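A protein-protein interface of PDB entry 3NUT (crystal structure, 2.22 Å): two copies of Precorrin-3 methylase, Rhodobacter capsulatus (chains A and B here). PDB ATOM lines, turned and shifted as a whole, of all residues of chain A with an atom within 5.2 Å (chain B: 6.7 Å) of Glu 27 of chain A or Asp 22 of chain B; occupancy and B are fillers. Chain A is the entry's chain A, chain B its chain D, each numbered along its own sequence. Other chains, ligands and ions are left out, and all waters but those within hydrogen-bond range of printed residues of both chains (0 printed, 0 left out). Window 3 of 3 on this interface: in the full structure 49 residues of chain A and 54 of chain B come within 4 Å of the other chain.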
ATOM      1  N   THR A  25      -0.861   0.057  16.296  1.00  0.00           N
ATOM      2  CA  THR A  25       0.152  -0.778  15.667  1.00  0.00           C
ATOM      3  C   THR A  25       1.524  -0.369  16.154  1.00  0.00           C
ATOM      4  O   THR A  25       1.711   0.777  16.508  1.00  0.00           O
ATOM      5  CB  THR A  25       0.073  -0.702  14.175  1.00  0.00           C
ATOM      6  OG1 THR A  25       0.336   0.653  13.766  1.00  0.00           O
ATOM      7  CG2 THR A  25      -1.281  -1.157  13.730  1.00  0.00           C
ATOM      8  N   PRO A  26       2.477  -1.313  16.233  1.00  0.00           N
ATOM      9  CA  PRO A  26       3.857  -0.922  16.554  1.00  0.00           C
ATOM     10  C   PRO A  26       4.443   0.110  15.581  1.00  0.00           C
ATOM     11  O   PRO A  26       5.221   0.952  15.999  1.00  0.00           O
ATOM     12  CB  PRO A  26       4.619  -2.254  16.472  1.00  0.00           C
ATOM     13  CG  PRO A  26       3.511  -3.259  17.032  1.00  0.00           C
ATOM     14  CD  PRO A  26       2.287  -2.782  16.293  1.00  0.00           C
ATOM     15  N   GLU A  27       4.081   0.034  14.312  1.00  0.00           N
ATOM     16  CA  GLU A  27       4.484   1.049  13.316  1.00  0.00           C
ATOM     17  C   GLU A  27       4.040   2.451  13.754  1.00  0.00           C
ATOM     18  O   GLU A  27       4.829   3.419  13.660  1.00  0.00           O
ATOM     19  CB  GLU A  27       3.885   0.695  11.941  1.00  0.00           C
ATOM     20  CG  GLU A  27       3.834   1.871  10.932  1.00  0.00           C
ATOM     21  CD  GLU A  27       3.491   1.459   9.499  1.00  0.00           C
ATOM     22  OE1 GLU A  27       2.336   1.603   9.037  1.00  0.00           O
ATOM     23  OE2 GLU A  27       4.400   1.002   8.810  1.00  0.00           O
ATOM     24  N   VAL A  28       2.782   2.562  14.243  1.00  0.00           N
ATOM     25  CA  VAL A  28       2.255   3.857  14.697  1.00  0.00           C
ATOM     26  C   VAL A  28       2.913   4.258  16.020  1.00  0.00           C
ATOM     27  O   VAL A  28       3.344   5.392  16.171  1.00  0.00           O
ATOM     28  CB  VAL A  28       0.688   3.961  14.730  1.00  0.00           C
ATOM     29  CG1 VAL A  28       0.227   5.221  15.512  1.00  0.00           C
ATOM     30  CG2 VAL A  28       0.111   3.970  13.324  1.00  0.00           C
ATOM     31  N   THR A  29       3.027   3.333  16.971  1.00  0.00           N
ATOM     32  CA  THR A  29       3.769   3.668  18.193  1.00  0.00           C
ATOM     33  C   THR A  29       5.206   4.217  17.850  1.00  0.00           C
ATOM     34  O   THR A  29       5.677   5.134  18.507  1.00  0.00           O
ATOM     35  CB  THR A  29       3.828   2.481  19.154  1.00  0.00           C
ATOM     36  OG1 THR A  29       2.491   2.175  19.619  1.00  0.00           O
ATOM     37  CG2 THR A  29       4.769   2.765  20.397  1.00  0.00           C
ATOM     38  N   ALA A  30       5.867   3.652  16.842  1.00  0.00           N
ATOM     39  CA  ALA A  30       7.229   4.094  16.448  1.00  0.00           C
ATOM     40  C   ALA A  30       7.274   5.486  15.785  1.00  0.00           C
ATOM     41  O   ALA A  30       8.191   6.259  16.053  1.00  0.00           O
ATOM     42  CB  ALA A  30       7.905   3.050  15.550  1.00  0.00           C
ATOM     43  N   ALA A  31       6.298   5.804  14.925  1.00  0.00           N
ATOM     44  CA  ALA A  31       6.172   7.157  14.369  1.00  0.00           C
ATOM     45  C   ALA A  31       5.962   8.212  15.474  1.00  0.00           C
ATOM     46  O   ALA A  31       6.559   9.297  15.449  1.00  0.00           O
ATOM     47  CB  ALA A  31       5.020   7.223  13.344  1.00  0.00           C
ATOM     48  N   ILE A 115       1.295   7.426   5.275  1.00  0.00           N
ATOM     49  CA  ILE A 115      -0.039   7.183   5.808  1.00  0.00           C
ATOM     50  C   ILE A 115      -0.011   5.816   6.504  1.00  0.00           C
ATOM     51  O   ILE A 115       0.253   4.798   5.861  1.00  0.00           O
ATOM     52  CB  ILE A 115      -1.099   7.168   4.671  1.00  0.00           C
ATOM     53  CG1 ILE A 115      -0.971   8.431   3.792  1.00  0.00           C
ATOM     54  CG2 ILE A 115      -2.578   7.016   5.253  1.00  0.00           C
ATOM     55  CD1 ILE A 115      -1.477   9.733   4.479  1.00  0.00           C
ATOM     56  N   LEU A 116      -0.271   5.810   7.820  1.00  0.00           N
ATOM     57  CA  LEU A 116      -0.116   4.621   8.657  1.00  0.00           C
ATOM     58  C   LEU A 116      -1.482   4.123   9.134  1.00  0.00           C
ATOM     59  O   LEU A 116      -2.172   4.830   9.867  1.00  0.00           O
ATOM     60  CB  LEU A 116       0.792   4.947   9.858  1.00  0.00           C
ATOM     61  CG  LEU A 116       2.155   5.555   9.461  1.00  0.00           C
ATOM     62  CD1 LEU A 116       3.021   5.671  10.727  1.00  0.00           C
ATOM     63  CD2 LEU A 116       2.866   4.677   8.393  1.00  0.00           C
ATOM     64  N   PRO A 117      -1.878   2.924   8.701  1.00  0.00           N
ATOM     65  CA  PRO A 117      -3.221   2.413   8.952  1.00  0.00           C
ATOM     66  C   PRO A 117      -3.486   2.143  10.427  1.00  0.00           C
ATOM     67  O   PRO A 117      -2.544   2.081  11.211  1.00  0.00           O
ATOM     68  CB  PRO A 117      -3.278   1.094   8.141  1.00  0.00           C
ATOM     69  CG  PRO A 117      -1.856   0.749   7.784  1.00  0.00           C
ATOM     70  CD  PRO A 117      -1.126   2.093   7.740  1.00  0.00           C
ATOM     71  N   GLY B  19       0.769  -8.432   6.488  1.00  0.00           N
ATOM     72  CA  GLY B  19       2.051  -9.126   6.340  1.00  0.00           C
ATOM     73  C   GLY B  19       3.158  -8.628   7.244  1.00  0.00           C
ATOM     74  O   GLY B  19       3.833  -9.419   7.873  1.00  0.00           O
ATOM     75  N   ARG B  20       3.356  -7.322   7.331  1.00  0.00           N
ATOM     76  CA  ARG B  20       4.457  -6.819   8.141  1.00  0.00           C
ATOM     77  C   ARG B  20       4.166  -6.975   9.643  1.00  0.00           C
ATOM     78  O   ARG B  20       3.072  -6.682  10.111  1.00  0.00           O
ATOM     79  CB  ARG B  20       4.814  -5.363   7.769  1.00  0.00           C
ATOM     80  CG  ARG B  20       6.321  -5.078   7.699  1.00  0.00           C
ATOM     81  CD  ARG B  20       6.646  -3.531   7.752  1.00  0.00           C
ATOM     82  NE  ARG B  20       5.853  -2.870   6.740  1.00  0.00           N
ATOM     83  CZ  ARG B  20       4.885  -1.984   6.969  1.00  0.00           C
ATOM     84  NH1 ARG B  20       4.609  -1.569   8.200  1.00  0.00           N
ATOM     85  NH2 ARG B  20       4.200  -1.515   5.941  1.00  0.00           N
ATOM     86  N   GLU B  21       5.171  -7.416  10.386  1.00  0.00           N
ATOM     87  CA  GLU B  21       5.053  -7.769  11.781  1.00  0.00           C
ATOM     88  C   GLU B  21       4.733  -6.548  12.651  1.00  0.00           C
ATOM     89  O   GLU B  21       4.109  -6.660  13.732  1.00  0.00           O
ATOM     90  CB  GLU B  21       6.368  -8.412  12.206  1.00  0.00           C
ATOM     91  CG  GLU B  21       6.496  -8.883  13.651  1.00  0.00           C
ATOM     92  CD  GLU B  21       7.549  -9.992  13.774  1.00  0.00           C
ATOM     93  OE1 GLU B  21       7.455 -10.971  12.977  1.00  0.00           O
ATOM     94  OE2 GLU B  21       8.465  -9.890  14.635  1.00  0.00           O
ATOM     95  N   ASP B  22       5.127  -5.373  12.185  1.00  0.00           N
ATOM     96  CA  ASP B  22       4.826  -4.172  12.933  1.00  0.00           C
ATOM     97  C   ASP B  22       3.370  -3.661  12.721  1.00  0.00           C
ATOM     98  O   ASP B  22       3.009  -2.576  13.146  1.00  0.00           O
ATOM     99  CB  ASP B  22       5.883  -3.108  12.661  1.00  0.00           C
ATOM    100  CG  ASP B  22       5.864  -2.621  11.230  1.00  0.00           C
ATOM    101  OD1 ASP B  22       5.039  -3.130  10.436  1.00  0.00           O
ATOM    102  OD2 ASP B  22       6.667  -1.699  10.910  1.00  0.00           O
ATOM    103  N   LEU B  23       2.536  -4.473  12.090  1.00  0.00           N
ATOM    104  CA  LEU B  23       1.111  -4.167  11.980  1.00  0.00           C
ATOM    105  C   LEU B  23       0.246  -5.071  12.846  1.00  0.00           C
ATOM    106  O   LEU B  23      -0.989  -4.860  12.927  1.00  0.00           O
ATOM    107  CB  LEU B  23       0.669  -4.242  10.516  1.00  0.00           C
ATOM    108  CG  LEU B  23       1.372  -3.199   9.620  1.00  0.00           C
ATOM    109  CD1 LEU B  23       1.064  -3.403   8.160  1.00  0.00           C
ATOM    110  CD2 LEU B  23       1.003  -1.789  10.044  1.00  0.00           C
ATOM    111  N   VAL B  24       0.871  -6.083  13.472  1.00  0.00           N
ATOM    112  CA  VAL B  24       0.142  -7.019  14.347  1.00  0.00           C
ATOM    113  C   VAL B  24      -0.177  -6.231  15.624  1.00  0.00           C
ATOM    114  O   VAL B  24       0.733  -5.729  16.293  1.00  0.00           O
ATOM    115  CB  VAL B  24       0.980  -8.258  14.668  1.00  0.00           C
ATOM    116  CG1 VAL B  24       0.274  -9.195  15.671  1.00  0.00           C
ATOM    117  CG2 VAL B  24       1.396  -9.029  13.390  1.00  0.00           C
ATOM    118  N   THR B  25      -1.448  -6.099  15.984  1.00  0.00           N
ATOM    119  CA  THR B  25      -1.758  -5.373  17.216  1.00  0.00           C
ATOM    120  C   THR B  25      -1.087  -6.056  18.421  1.00  0.00           C
ATOM    121  O   THR B  25      -0.838  -7.272  18.381  1.00  0.00           O
ATOM    122  CB  THR B  25      -3.267  -5.296  17.494  1.00  0.00           C
ATOM    123  OG1 THR B  25      -3.752  -6.620  17.766  1.00  0.00           O
ATOM    124  CG2 THR B  25      -3.989  -4.679  16.332  1.00  0.00           C
ATOM    125  N   THR B 204       2.726  -4.099   1.995  1.00  0.00           N
ATOM    126  CA  THR B 204       3.505  -4.095   3.243  1.00  0.00           C
ATOM    127  C   THR B 204       4.657  -5.077   3.274  1.00  0.00           C
ATOM    128  O   THR B 204       5.488  -4.991   4.146  1.00  0.00           O
ATOM    129  CB  THR B 204       2.658  -4.249   4.585  1.00  0.00           C
ATOM    130  OG1 THR B 204       2.240  -5.604   4.761  1.00  0.00           O
ATOM    131  CG2 THR B 204       1.467  -3.317   4.608  1.00  0.00           C
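1 position is printed for both chains.
Of the 7 pairs that touch across the chains among the printed residues, none has its exchanged pair printed and touching as well.
O of Asp 22 of chain B is in hydrogen-bond range of N of Glu 27 of chain A (3.1 Å).
N of Pro 26 of chain A sits close to O of Asp 22 of chain B, 3.4 Å away.
The side-chain carboxylate (OE2) of Glu 27 of chain A lies within salt-bridge range of the guanidinium group (NH1) of Arg 20 of chain B, at 2.7 Å.
OG1 of Thr 204 of chain B is in hydrogen-bond range of N of Arg 20 of chain B (3.3 Å).
The backbone carbonyl oxygen of Thr 25 of chain A is in hydrogen-bond range of the side-chain hydroxyl of Thr 29 of chain A, 3.5 Å away.
OD1 of Asp 22 of chain B is in salt-bridge range of NH1 of Arg 20 of chain B (2.8 Å).
N of Val 28 of chain A sits at hydrogen-bond distance from OG1 of Thr 25 of chain A (3.1 Å).
CB of Thr 25 of chain A touches O of Asp 22 of chain B, 3.6 Å away.
Thr 25 of chain A touches Leu 23 of chain B.
Val 24 of chain B touches Pro 26 of chain A.
Glu 27 of chain A touches Leu 23 of chain B (OE1 to CD2, 3.8 Å).
Glu 27 of chain A touches three residues of chain B.
Of chain A, only Thr 25 (3.6 Å), Pro 26 (3.2 Å) and Glu 27 (3.1 Å) come within 4 Å of Asp 22 of chain B.
Of the printed residues of chain A, Arg 20 of chain B touches Glu 27 (2.7 Å).
Of the printed residues of chain B, Pro 26 of chain A touches Asp 22 (3.2 Å) and Val 24 (3.3 Å).
Printed residues of chain A within 4 Å of Val 24 of chain B: Pro 26 (3.3 Å).
Printed residues of chain B within 4 Å of Thr 25 of chain A: Asp 22 (3.6 Å) and Leu 23 (3.8 Å).
The nearest printed residue of chain B that does not touch Glu 27 of chain A is Thr 204 of chain B (6.7 Å).
Of the 10 printed residues of chain A, 3 touch a printed residue of chain B.
Printed residues of chain A that touch a printed residue of chain B: Thr 25, Pro 26 and Glu 27.
Hydrophobic or aromatic side chains of chain A that line the printed part of chain B: Pro 26.
Of the 8 printed residues of chain B, 4 touch a printed residue of chain A.
Printed residues of chain B that touch a printed residue of chain A: Arg 20, Asp 22, Leu 23 and Val 24.
Hydrophobic or aromatic side chains of chain B that line the printed part of chain A: Leu 23.
Among the printed residues, Asp or Glu carboxylates within 4 Å of a Lys or Arg side-chain nitrogen of the other chain: Glu 27 of chain A with Arg 20 of chain B.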
